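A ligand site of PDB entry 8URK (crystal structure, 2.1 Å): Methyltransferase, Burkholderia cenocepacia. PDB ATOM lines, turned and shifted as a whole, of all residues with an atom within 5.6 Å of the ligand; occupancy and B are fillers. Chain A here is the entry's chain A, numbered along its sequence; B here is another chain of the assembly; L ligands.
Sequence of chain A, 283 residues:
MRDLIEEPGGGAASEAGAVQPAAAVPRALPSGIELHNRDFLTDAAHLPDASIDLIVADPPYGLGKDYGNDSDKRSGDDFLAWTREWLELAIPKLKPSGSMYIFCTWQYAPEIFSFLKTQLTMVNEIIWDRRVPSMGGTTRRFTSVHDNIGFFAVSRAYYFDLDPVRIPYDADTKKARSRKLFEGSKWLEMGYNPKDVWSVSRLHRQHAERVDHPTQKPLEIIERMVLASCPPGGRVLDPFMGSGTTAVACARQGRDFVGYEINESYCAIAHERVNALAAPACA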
ATOM      1  N   ARG A  38      22.797   0.162  26.218  1.00  0.00           N
ATOM      2  CA  ARG A  38      22.024  -1.040  26.450  1.00  0.00           C
ATOM      3  C   ARG A  38      21.539  -1.729  25.184  1.00  0.00           C
ATOM      4  O   ARG A  38      21.397  -1.095  24.146  1.00  0.00           O
ATOM      5  CB  ARG A  38      20.816  -0.687  27.296  1.00  0.00           C
ATOM      6  CG  ARG A  38      21.109  -0.553  28.780  1.00  0.00           C
ATOM      7  N   ASP A  39      21.250  -3.015  25.261  1.00  0.00           N
ATOM      8  CA  ASP A  39      20.701  -3.730  24.141  1.00  0.00           C
ATOM      9  C   ASP A  39      19.288  -3.252  23.905  1.00  0.00           C
ATOM     10  O   ASP A  39      18.482  -3.271  24.807  1.00  0.00           O
ATOM     11  CB  ASP A  39      20.754  -5.227  24.423  1.00  0.00           C
ATOM     12  CG  ASP A  39      19.964  -6.067  23.420  1.00  0.00           C
ATOM     13  OD1 ASP A  39      19.287  -5.549  22.529  1.00  0.00           O
ATOM     14  OD2 ASP A  39      20.030  -7.306  23.542  1.00  0.00           O
ATOM     15  N   PHE A  40      18.987  -2.872  22.674  1.00  0.00           N
ATOM     16  CA  PHE A  40      17.668  -2.344  22.357  1.00  0.00           C
ATOM     17  C   PHE A  40      16.539  -3.329  22.510  1.00  0.00           C
ATOM     18  O   PHE A  40      15.455  -2.940  22.869  1.00  0.00           O
ATOM     19  CB  PHE A  40      17.675  -1.774  20.936  1.00  0.00           C
ATOM     20  CG  PHE A  40      16.330  -1.376  20.441  1.00  0.00           C
ATOM     21  CD1 PHE A  40      15.806  -0.136  20.738  1.00  0.00           C
ATOM     22  CD2 PHE A  40      15.595  -2.241  19.660  1.00  0.00           C
ATOM     23  CE1 PHE A  40      14.561   0.234  20.273  1.00  0.00           C
ATOM     24  CE2 PHE A  40      14.351  -1.876  19.187  1.00  0.00           C
ATOM     25  CZ  PHE A  40      13.833  -0.636  19.497  1.00  0.00           C
ATOM     26  N   LEU A  41      16.774  -4.586  22.226  1.00  0.00           N
ATOM     27  CA  LEU A  41      15.698  -5.554  22.260  1.00  0.00           C
ATOM     28  C   LEU A  41      15.252  -5.870  23.679  1.00  0.00           C
ATOM     29  O   LEU A  41      14.136  -6.262  23.895  1.00  0.00           O
ATOM     30  CB  LEU A  41      16.106  -6.822  21.530  1.00  0.00           C
ATOM     31  CG  LEU A  41      16.177  -6.706  20.000  1.00  0.00           C
ATOM     32  CD1 LEU A  41      17.528  -6.180  19.563  1.00  0.00           C
ATOM     33  CD2 LEU A  41      15.880  -8.046  19.361  1.00  0.00           C
ATOM     34  N   ASP A  58      20.239   2.430  11.507  1.00  0.00           N
ATOM     35  CA  ASP A  58      21.323   1.924  10.702  1.00  0.00           C
ATOM     36  C   ASP A  58      21.726   0.642  11.369  1.00  0.00           C
ATOM     37  O   ASP A  58      22.747   0.548  12.015  1.00  0.00           O
ATOM     38  CB  ASP A  58      22.465   2.916  10.597  1.00  0.00           C
ATOM     39  CG  ASP A  58      23.670   2.348   9.861  1.00  0.00           C
ATOM     40  OD1 ASP A  58      23.509   1.400   9.080  1.00  0.00           O
ATOM     41  OD2 ASP A  58      24.771   2.878  10.073  1.00  0.00           O
ATOM     42  N   PRO A  59      20.916  -0.380  11.188  1.00  0.00           N
ATOM     43  CA  PRO A  59      21.177  -1.636  11.863  1.00  0.00           C
ATOM     44  C   PRO A  59      22.269  -2.473  11.197  1.00  0.00           C
ATOM     45  O   PRO A  59      22.671  -2.164  10.098  1.00  0.00           O
ATOM     46  CB  PRO A  59      19.867  -2.349  11.704  1.00  0.00           C
ATOM     47  CG  PRO A  59      19.354  -1.896  10.387  1.00  0.00           C
ATOM     48  CD  PRO A  59      19.792  -0.471  10.258  1.00  0.00           C
ATOM     49  N   PRO A  60      22.733  -3.520  11.875  1.00  0.00           N
ATOM     50  CA  PRO A  60      23.696  -4.397  11.191  1.00  0.00           C
ATOM     51  C   PRO A  60      23.124  -4.897   9.857  1.00  0.00           C
ATOM     52  O   PRO A  60      22.014  -5.341   9.806  1.00  0.00           O
ATOM     53  CB  PRO A  60      23.906  -5.539  12.180  1.00  0.00           C
ATOM     54  CG  PRO A  60      22.877  -5.367  13.233  1.00  0.00           C
ATOM     55  CD  PRO A  60      22.526  -3.918  13.271  1.00  0.00           C
ATOM     56  N   TYR A  67      31.810  -5.534  15.001  1.00  0.00           N
ATOM     57  CA  TYR A  67      31.367  -4.432  15.815  1.00  0.00           C
ATOM     58  C   TYR A  67      31.767  -4.632  17.270  1.00  0.00           C
ATOM     59  O   TYR A  67      31.262  -3.943  18.137  1.00  0.00           O
ATOM     60  CB  TYR A  67      29.839  -4.350  15.728  1.00  0.00           C
ATOM     61  CG  TYR A  67      29.253  -3.724  14.489  1.00  0.00           C
ATOM     62  CD1 TYR A  67      29.846  -2.620  13.889  1.00  0.00           C
ATOM     63  CD2 TYR A  67      28.077  -4.210  13.942  1.00  0.00           C
ATOM     64  CE1 TYR A  67      29.283  -2.042  12.771  1.00  0.00           C
ATOM     65  CE2 TYR A  67      27.524  -3.642  12.820  1.00  0.00           C
ATOM     66  CZ  TYR A  67      28.129  -2.556  12.246  1.00  0.00           C
ATOM     67  OH  TYR A  67      27.576  -1.988  11.124  1.00  0.00           O
ATOM     68  N   ASN A  69      31.213  -7.407  18.524  1.00  0.00           N
ATOM     69  CA  ASN A  69      30.231  -8.386  18.878  1.00  0.00           C
ATOM     70  C   ASN A  69      29.778  -9.093  17.608  1.00  0.00           C
ATOM     71  O   ASN A  69      30.331  -8.875  16.543  1.00  0.00           O
ATOM     72  CB  ASN A  69      29.052  -7.719  19.558  1.00  0.00           C
ATOM     73  CG  ASN A  69      28.565  -6.508  18.796  1.00  0.00           C
ATOM     74  OD1 ASN A  69      27.883  -6.628  17.787  1.00  0.00           O
ATOM     75  ND2 ASN A  69      28.915  -5.324  19.281  1.00  0.00           N
ATOM     76  N   SER A  71      26.722  -8.954  16.146  1.00  0.00           N
ATOM     77  CA  SER A  71      25.511  -8.372  15.604  1.00  0.00           C
ATOM     78  C   SER A  71      25.451  -8.555  14.098  1.00  0.00           C
ATOM     79  O   SER A  71      24.410  -8.889  13.572  1.00  0.00           O
ATOM     80  CB  SER A  71      25.450  -6.890  15.969  1.00  0.00           C
ATOM     81  OG  SER A  71      26.554  -6.174  15.473  1.00  0.00           O
ATOM     82  N   TRP A  82      15.929 -11.971  12.806  1.00  0.00           N
ATOM     83  CA  TRP A  82      16.329 -10.992  13.820  1.00  0.00           C
ATOM     84  C   TRP A  82      15.881  -9.587  13.427  1.00  0.00           C
ATOM     85  O   TRP A  82      15.452  -8.805  14.278  1.00  0.00           O
ATOM     86  CB  TRP A  82      17.842 -11.053  14.034  1.00  0.00           C
ATOM     87  CG  TRP A  82      18.340  -9.999  14.964  1.00  0.00           C
ATOM     88  CD1 TRP A  82      18.368 -10.048  16.318  1.00  0.00           C
ATOM     89  CD2 TRP A  82      18.894  -8.723  14.595  1.00  0.00           C
ATOM     90  NE1 TRP A  82      18.889  -8.887  16.835  1.00  0.00           N
ATOM     91  CE2 TRP A  82      19.218  -8.048  15.794  1.00  0.00           C
ATOM     92  CE3 TRP A  82      19.140  -8.087  13.385  1.00  0.00           C
ATOM     93  CZ2 TRP A  82      19.784  -6.780  15.808  1.00  0.00           C
ATOM     94  CZ3 TRP A  82      19.699  -6.826  13.401  1.00  0.00           C
ATOM     95  CH2 TRP A  82      20.015  -6.187  14.597  1.00  0.00           C
ATOM     96  N   HIS A 213      34.963   3.905  14.583  1.00  0.00           N
ATOM     97  CA  HIS A 213      33.858   3.002  14.339  1.00  0.00           C
ATOM     98  C   HIS A 213      33.978   2.456  12.914  1.00  0.00           C
ATOM     99  O   HIS A 213      34.349   3.185  12.026  1.00  0.00           O
ATOM    100  CB  HIS A 213      32.538   3.694  14.474  1.00  0.00           C
ATOM    101  CG  HIS A 213      31.356   2.794  14.488  1.00  0.00           C
ATOM    102  ND1 HIS A 213      30.631   2.504  13.346  1.00  0.00           N
ATOM    103  CD2 HIS A 213      30.757   2.117  15.493  1.00  0.00           C
ATOM    104  CE1 HIS A 213      29.642   1.689  13.655  1.00  0.00           C
ATOM    105  NE2 HIS A 213      29.699   1.430  14.956  1.00  0.00           N
ATOM    106  N   THR A 215      31.602   1.342  10.731  1.00  0.00           N
ATOM    107  CA  THR A 215      30.546   1.663   9.799  1.00  0.00           C
ATOM    108  C   THR A 215      29.893   3.021  10.038  1.00  0.00           C
ATOM    109  O   THR A 215      28.709   3.119  10.182  1.00  0.00           O
ATOM    110  CB  THR A 215      29.489   0.558   9.828  1.00  0.00           C
ATOM    111  OG1 THR A 215      28.919   0.451  11.133  1.00  0.00           O
ATOM    112  CG2 THR A 215      30.109  -0.780   9.411  1.00  0.00           C
ATOM    113  N   GLN A 216      30.696   4.053  10.078  1.00  0.00           N
ATOM    114  CA  GLN A 216      30.198   5.380  10.326  1.00  0.00           C
ATOM    115  C   GLN A 216      29.335   5.887   9.204  1.00  0.00           C
ATOM    116  O   GLN A 216      29.370   5.369   8.115  1.00  0.00           O
ATOM    117  CB  GLN A 216      31.350   6.343  10.543  1.00  0.00           C
ATOM    118  CG  GLN A 216      31.123   7.286  11.716  1.00  0.00           C
ATOM    119  CD  GLN A 216      32.217   8.325  11.871  1.00  0.00           C
ATOM    120  OE1 GLN A 216      33.391   7.997  11.893  1.00  0.00           O
ATOM    121  NE2 GLN A 216      31.817   9.572  11.976  1.00  0.00           N
ATOM    122  N   LYS A 217      28.554   6.899   9.498  1.00  0.00           N
ATOM    123  CA  LYS A 217      27.685   7.452   8.514  1.00  0.00           C
ATOM    124  C   LYS A 217      27.862   8.948   8.469  1.00  0.00           C
ATOM    125  O   LYS A 217      27.849   9.607   9.488  1.00  0.00           O
ATOM    126  CB  LYS A 217      26.257   7.044   8.797  1.00  0.00           C
ATOM    127  CG  LYS A 217      25.996   5.565   8.676  1.00  0.00           C
ATOM    128  CD  LYS A 217      25.718   5.157   7.236  1.00  0.00           C
ATOM    129  CE  LYS A 217      25.427   3.680   7.119  1.00  0.00           C
ATOM    130  NZ  LYS A 217      26.531   2.884   7.698  1.00  0.00           N
ATOM    131  N   ASP A 238      17.245   6.066  17.791  1.00  0.00           N
ATOM    132  CA  ASP A 238      18.201   5.326  16.994  1.00  0.00           C
ATOM    133  C   ASP A 238      18.509   4.006  17.697  1.00  0.00           C
ATOM    134  O   ASP A 238      19.351   3.948  18.579  1.00  0.00           O
ATOM    135  CB  ASP A 238      19.468   6.130  16.759  1.00  0.00           C
ATOM    136  CG  ASP A 238      20.448   5.428  15.824  1.00  0.00           C
ATOM    137  OD1 ASP A 238      20.356   4.203  15.657  1.00  0.00           O
ATOM    138  OD2 ASP A 238      21.313   6.107  15.268  1.00  0.00           O
ATOM    139  N   PRO A 239      17.862   2.929  17.265  1.00  0.00           N
ATOM    140  CA  PRO A 239      18.039   1.643  17.950  1.00  0.00           C
ATOM    141  C   PRO A 239      19.477   1.095  17.995  1.00  0.00           C
ATOM    142  O   PRO A 239      19.767   0.308  18.865  1.00  0.00           O
ATOM    143  CB  PRO A 239      17.119   0.712  17.166  1.00  0.00           C
ATOM    144  CG  PRO A 239      16.168   1.599  16.459  1.00  0.00           C
ATOM    145  CD  PRO A 239      16.928   2.837  16.141  1.00  0.00           C
ATOM    146  N   PHE A 240      20.345   1.520  17.094  1.00  0.00           N
ATOM    147  CA  PHE A 240      21.732   1.066  17.067  1.00  0.00           C
ATOM    148  C   PHE A 240      22.589   2.241  16.644  1.00  0.00           C
ATOM    149  O   PHE A 240      23.041   2.319  15.522  1.00  0.00           O
ATOM    150  CB  PHE A 240      21.866  -0.139  16.146  1.00  0.00           C
ATOM    151  CG  PHE A 240      20.740  -1.122  16.238  1.00  0.00           C
ATOM    152  CD1 PHE A 240      20.712  -2.069  17.239  1.00  0.00           C
ATOM    153  CD2 PHE A 240      19.724  -1.104  15.302  1.00  0.00           C
ATOM    154  CE1 PHE A 240      19.677  -2.969  17.325  1.00  0.00           C
ATOM    155  CE2 PHE A 240      18.684  -2.016  15.383  1.00  0.00           C
ATOM    156  CZ  PHE A 240      18.662  -2.951  16.390  1.00  0.00           C
ATOM    157  N   MET A 241      22.831   3.154  17.576  1.00  0.00           N
ATOM    158  CA  MET A 241      23.511   4.411  17.250  1.00  0.00           C
ATOM    159  C   MET A 241      24.999   4.425  16.965  1.00  0.00           C
ATOM    160  O   MET A 241      25.506   5.391  16.430  1.00  0.00           O
ATOM    161  CB  MET A 241      23.233   5.371  18.412  1.00  0.00           C
ATOM    162  CG  MET A 241      23.941   5.010  19.706  1.00  0.00           C
ATOM    163  SD  MET A 241      23.858   6.327  20.931  1.00  0.00           S
ATOM    164  CE  MET A 241      24.982   5.724  22.166  1.00  0.00           C
ATOM    165  N   GLY A 242      25.700   3.388  17.332  1.00  0.00           N
ATOM    166  CA  GLY A 242      27.103   3.365  17.110  1.00  0.00           C
ATOM    167  C   GLY A 242      27.827   4.553  17.647  1.00  0.00           C
ATOM    168  O   GLY A 242      27.935   4.684  18.847  1.00  0.00           O
ATOM    169  N   SER A 243      28.310   5.429  16.789  1.00  0.00           N
ATOM    170  CA  SER A 243      29.096   6.579  17.198  1.00  0.00           C
ATOM    171  C   SER A 243      28.273   7.809  17.573  1.00  0.00           C
ATOM    172  O   SER A 243      28.824   8.858  17.770  1.00  0.00           O
ATOM    173  CB  SER A 243      30.045   6.960  16.054  1.00  0.00           C
ATOM    174  OG  SER A 243      30.925   5.910  15.760  1.00  0.00           O
ATOM    175  N   GLY A 244      26.975   7.654  17.643  1.00  0.00           N
ATOM    176  CA  GLY A 244      26.095   8.751  17.943  1.00  0.00           C
ATOM    177  C   GLY A 244      25.967   9.773  16.856  1.00  0.00           C
ATOM    178  O   GLY A 244      25.726  10.931  17.129  1.00  0.00           O
ATOM    179  N   THR A 245      26.135   9.355  15.615  1.00  0.00           N
ATOM    180  CA  THR A 245      25.989  10.259  14.514  1.00  0.00           C
ATOM    181  C   THR A 245      24.622  10.919  14.561  1.00  0.00           C
ATOM    182  O   THR A 245      24.509  12.106  14.376  1.00  0.00           O
ATOM    183  CB  THR A 245      26.227   9.564  13.152  1.00  0.00           C
ATOM    184  OG1 THR A 245      27.493   8.894  13.159  1.00  0.00           O
ATOM    185  CG2 THR A 245      26.211  10.563  12.022  1.00  0.00           C
ATOM    186  N   THR A 246      23.593  10.141  14.825  1.00  0.00           N
ATOM    187  CA  THR A 246      22.252  10.696  14.932  1.00  0.00           C
ATOM    188  C   THR A 246      22.163  11.640  16.150  1.00  0.00           C
ATOM    189  O   THR A 246      21.560  12.691  16.064  1.00  0.00           O
ATOM    190  CB  THR A 246      21.207   9.564  14.956  1.00  0.00           C
ATOM    191  OG1 THR A 246      21.722   8.426  14.267  1.00  0.00           O
ATOM    192  CG2 THR A 246      19.941  10.015  14.278  1.00  0.00           C
ATOM    193  N   TYR A 260      20.550   3.553  21.609  1.00  0.00           N
ATOM    194  CA  TYR A 260      21.126   2.400  22.260  1.00  0.00           C
ATOM    195  C   TYR A 260      22.322   1.808  21.512  1.00  0.00           C
ATOM    196  O   TYR A 260      22.291   1.700  20.306  1.00  0.00           O
ATOM    197  CB  TYR A 260      20.056   1.335  22.429  1.00  0.00           C
ATOM    198  CG  TYR A 260      18.830   1.782  23.176  1.00  0.00           C
ATOM    199  CD1 TYR A 260      17.920   2.647  22.589  1.00  0.00           C
ATOM    200  CD2 TYR A 260      18.570   1.328  24.449  1.00  0.00           C
ATOM    201  CE1 TYR A 260      16.797   3.053  23.266  1.00  0.00           C
ATOM    202  CE2 TYR A 260      17.448   1.723  25.134  1.00  0.00           C
ATOM    203  CZ  TYR A 260      16.561   2.591  24.538  1.00  0.00           C
ATOM    204  OH  TYR A 260      15.433   2.997  25.202  1.00  0.00           O
ATOM    205  N   GLU A 261      23.377   1.466  22.240  1.00  0.00           N
ATOM    206  CA  GLU A 261      24.558   0.849  21.650  1.00  0.00           C
ATOM    207  C   GLU A 261      25.200  -0.098  22.621  1.00  0.00           C
ATOM    208  O   GLU A 261      25.681   0.314  23.650  1.00  0.00           O
ATOM    209  CB  GLU A 261      25.589   1.866  21.223  1.00  0.00           C
ATOM    210  CG  GLU A 261      26.964   1.311  20.944  1.00  0.00           C
ATOM    211  CD  GLU A 261      26.960   0.352  19.785  1.00  0.00           C
ATOM    212  OE1 GLU A 261      26.672   0.776  18.662  1.00  0.00           O
ATOM    213  OE2 GLU A 261      27.244  -0.836  19.988  1.00  0.00           O
ATOM    214  N   ILE A 262      25.195  -1.376  22.316  1.00  0.00           N
ATOM    215  CA  ILE A 262      25.805  -2.368  23.164  1.00  0.00           C
ATOM    216  C   ILE A 262      27.275  -2.121  23.427  1.00  0.00           C
ATOM    217  O   ILE A 262      27.704  -2.246  24.553  1.00  0.00           O
ATOM    218  CB  ILE A 262      25.603  -3.761  22.557  1.00  0.00           C
ATOM    219  CG1 ILE A 262      25.942  -3.748  21.062  1.00  0.00           C
ATOM    220  CG2 ILE A 262      24.174  -4.230  22.758  1.00  0.00           C
ATOM    221  CD1 ILE A 262      25.759  -5.095  20.394  1.00  0.00           C
ATOM    222  N   ASN A 263      28.036  -1.771  22.402  1.00  0.00           N
ATOM    223  CA  ASN A 263      29.445  -1.500  22.575  1.00  0.00           C
ATOM    224  C   ASN A 263      29.651  -0.286  23.441  1.00  0.00           C
ATOM    225  O   ASN A 263      29.097   0.755  23.192  1.00  0.00           O
ATOM    226  CB  ASN A 263      30.145  -1.332  21.227  1.00  0.00           C
ATOM    227  CG  ASN A 263      31.648  -1.401  21.324  1.00  0.00           C
ATOM    228  OD1 ASN A 263      32.252  -0.772  22.173  1.00  0.00           O
ATOM    229  ND2 ASN A 263      32.246  -2.151  20.422  1.00  0.00           N
ATOM    230  N   TYR A 266      31.790   2.580  21.780  1.00  0.00           N
ATOM    231  CA  TYR A 266      31.013   3.377  20.870  1.00  0.00           C
ATOM    232  C   TYR A 266      30.221   4.408  21.668  1.00  0.00           C
ATOM    233  O   TYR A 266      30.226   5.582  21.339  1.00  0.00           O
ATOM    234  CB  TYR A 266      30.100   2.482  20.053  1.00  0.00           C
ATOM    235  CG  TYR A 266      30.791   1.501  19.126  1.00  0.00           C
ATOM    236  CD1 TYR A 266      32.149   1.583  18.875  1.00  0.00           C
ATOM    237  CD2 TYR A 266      30.073   0.480  18.508  1.00  0.00           C
ATOM    238  CE1 TYR A 266      32.779   0.682  18.039  1.00  0.00           C
ATOM    239  CE2 TYR A 266      30.688  -0.423  17.671  1.00  0.00           C
ATOM    240  CZ  TYR A 266      32.040  -0.313  17.436  1.00  0.00           C
ATOM    241  OH  TYR A 266      32.681  -1.206  16.611  1.00  0.00           O
ATOM    242  N   ARG A 273      31.539  12.896  21.137  1.00  0.00           N
ATOM    243  CA  ARG A 273      31.084  13.608  19.960  1.00  0.00           C
ATOM    244  C   ARG A 273      30.008  14.629  20.284  1.00  0.00           C
ATOM    245  O   ARG A 273      29.984  15.687  19.695  1.00  0.00           O
ATOM    246  CB  ARG A 273      30.570  12.597  18.915  1.00  0.00           C
ATOM    247  CG  ARG A 273      31.664  11.801  18.248  1.00  0.00           C
ATOM    248  CD  ARG A 273      31.580  11.919  16.740  1.00  0.00           C
ATOM    249  NE  ARG A 273      30.650  10.942  16.188  1.00  0.00           N
ATOM    250  CZ  ARG A 273      29.978  11.102  15.065  1.00  0.00           C
ATOM    251  NH1 ARG A 273      30.120  12.194  14.350  1.00  0.00           N
ATOM    252  NH2 ARG A 273      29.159  10.146  14.659  1.00  0.00           N
ATOM    253  P    DA B   7      32.707   2.951   5.614  1.00  0.00           P
ATOM    254  OP1  DA B   7      31.656   3.707   4.916  1.00  0.00           O
ATOM    255  OP2  DA B   7      33.081   3.334   6.972  1.00  0.00           O
ATOM    256  O5'  DA B   7      32.333   1.403   5.666  1.00  0.00           O
ATOM    257  C5'  DA B   7      31.569   0.789   4.636  1.00  0.00           C
ATOM    258  C4'  DA B   7      31.617  -0.715   4.776  1.00  0.00           C
ATOM    259  O4'  DA B   7      30.861  -1.105   5.936  1.00  0.00           O
ATOM    260  C3'  DA B   7      31.009  -1.489   3.619  1.00  0.00           C
ATOM    261  O3'  DA B   7      31.595  -2.782   3.563  1.00  0.00           O
ATOM    262  C2'  DA B   7      29.564  -1.620   4.048  1.00  0.00           C
ATOM    263  C1'  DA B   7      29.715  -1.838   5.539  1.00  0.00           C
ATOM    264  N9   DA B   7      28.580  -1.374   6.334  1.00  0.00           N
ATOM    265  C8   DA B   7      28.045  -0.108   6.370  1.00  0.00           C
ATOM    266  N7   DA B   7      27.020  -0.009   7.180  1.00  0.00           N
ATOM    267  C5   DA B   7      26.879  -1.274   7.715  1.00  0.00           C
ATOM    268  C6   DA B   7      25.978  -1.815   8.645  1.00  0.00           C
ATOM    269  N6   DA B   7      25.017  -1.109   9.232  1.00  0.00           N
ATOM    270  N1   DA B   7      26.116  -3.121   8.960  1.00  0.00           N
ATOM    271  C2   DA B   7      27.091  -3.826   8.375  1.00  0.00           C
ATOM    272  N3   DA B   7      27.996  -3.432   7.490  1.00  0.00           N
ATOM    273  C4   DA B   7      27.841  -2.129   7.197  1.00  0.00           C
HETATM  274  N1  LIG L   1      25.124   4.642  12.451  1.00  0.00           N
HETATM  275  C1  LIG L   1      26.236   4.321  13.300  1.00  0.00           C
HETATM  276  C2  LIG L   1      27.287   5.335  13.025  1.00  0.00           C
HETATM  277  O1  LIG L   1      28.307   5.351  13.723  1.00  0.00           O
HETATM  278  O2  LIG L   1      27.071   6.128  12.134  1.00  0.00           O
HETATM  279  C3  LIG L   1      26.675   2.892  13.053  1.00  0.00           C
HETATM  280  C4  LIG L   1      25.814   1.869  13.778  1.00  0.00           C
HETATM  281  C5  LIG L   1      26.094   0.489  13.220  1.00  0.00           C
HETATM  282  N2  LIG L   1      25.737   0.465  11.820  1.00  0.00           N
HETATM  283  C6  LIG L   1      25.266  -0.543  13.971  1.00  0.00           C
HETATM  284  C7  LIG L   1      25.581  -0.528  15.464  1.00  0.00           C
HETATM  285  O3  LIG L   1      24.554  -1.184  16.194  1.00  0.00           O
HETATM  286  C8  LIG L   1      26.861  -1.273  15.800  1.00  0.00           C
HETATM  287  O4  LIG L   1      27.792  -0.354  16.353  1.00  0.00           O
HETATM  288  C9  LIG L   1      26.474  -2.334  16.798  1.00  0.00           C
HETATM  289  O5  LIG L   1      27.432  -2.487  17.840  1.00  0.00           O
HETATM  290  C10 LIG L   1      25.156  -1.810  17.328  1.00  0.00           C
HETATM  291  N3  LIG L   1      24.269  -2.863  17.836  1.00  0.00           N
HETATM  292  C11 LIG L   1      24.212  -4.139  17.445  1.00  0.00           C
HETATM  293  N4  LIG L   1      23.267  -4.805  18.129  1.00  0.00           N
HETATM  294  C12 LIG L   1      22.703  -3.943  18.993  1.00  0.00           C
HETATM  295  C13 LIG L   1      21.642  -3.985  20.016  1.00  0.00           C
HETATM  296  N5  LIG L   1      20.961  -5.105  20.279  1.00  0.00           N
HETATM  297  N6  LIG L   1      21.369  -2.848  20.681  1.00  0.00           N
HETATM  298  C14 LIG L   1      22.030  -1.714  20.440  1.00  0.00           C
HETATM  299  N7  LIG L   1      23.000  -1.601  19.519  1.00  0.00           N
HETATM  300  C15 LIG L   1      23.375  -2.663  18.784  1.00  0.00           C
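OE2 of Glu 261 is in hydrogen-bond range of O5 of the ligand (2.7 Å).
OD1 of Asp 39 lies within hydrogen-bond range of N5 of the ligand, at 2.8 Å.
NE2 of His 213 sits at hydrogen-bond distance from O4 of the ligand, 3.0 Å away.
An oxygen (O2) of the ligand lies within hydrogen-bond range of the side-chain hydroxyl (OG1) of Thr 245 (3.0 Å).
The backbone carbonyl oxygen (O) of Asp 58 sits at hydrogen-bond distance from a nitrogen (N2) of the ligand (3.0 Å).
The side-chain carboxylate of Asp 58 is in salt-bridge range of a nitrogen (N1) of the ligand, at 3.0 Å.
An oxygen (O1) of the ligand sits at hydrogen-bond distance from the backbone NH (N) of Ser 243 (3.1 Å).
OG of Ser 243 lies close to O1 of the ligand, 3.4 Å away.
N of Phe 40 is in hydrogen-bond range of N6 of the ligand.
N2 of the ligand sits at hydrogen-bond distance from N6 of DA 7 of chain B (3.1 Å).
The backbone NH (N) of Lys 217 sits at hydrogen-bond distance from an oxygen (O2) of the ligand (3.1 Å).
OH of Tyr 67 is in hydrogen-bond range of N2 of the ligand, 3.1 Å away.
A nitrogen (N2) of the ligand is in hydrogen-bond range of the side-chain hydroxyl of Thr 215 (3.3 Å).
The backbone carbonyl oxygen (O) of Tyr 260 lies close to a nitrogen (N7) of the ligand (3.5 Å).
Residues that only touch the ligand: Phe 240 (2.9 Å), Tyr 266 (3.2 Å), Ser 71 (3.4 Å), Ile 262 (3.4 Å), Met 241 (3.4 Å), Pro 239 (3.4 Å), Asn 69 (3.5 Å), Leu 41 (3.7 Å), Gln 216 (3.7 Å), Arg 38 (3.8 Å) and Gly 242 (3.9 Å).
Of the 31 residues printed, 23 come within 4 Å of the ligand.
The nearest printed residue that does not touch the ligand is Pro 59 (4.4 Å).
The side-chain carboxylate of Glu 261 is in hydrogen-bond range of the backbone NH of Asn 263 (2.7 Å).
ND1 of His 213 is in hydrogen-bond range of N of Thr 215.
The side-chain hydroxyl of Thr 245 is in hydrogen-bond range of the guanidinium group of Arg 273, 2.6 Å away.
The backbone carbonyl oxygen (O) of Ser 243 lies within hydrogen-bond range of the guanidinium group (NE) of Arg 273.
N1 of DA 7 of chain B lies within hydrogen-bond range of the side-chain hydroxyl of Tyr 67, 2.8 Å away.
OH of Tyr 266 sits at hydrogen-bond distance from O of Tyr 67 (3.4 Å).
The side-chain amide nitrogen (ND2) of Asn 263 is in hydrogen-bond range of the backbone carbonyl oxygen (O) of Tyr 67 (3.1 Å).
OG of Ser 71 sits at hydrogen-bond distance from OD1 of Asn 69, at 2.7 Å.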
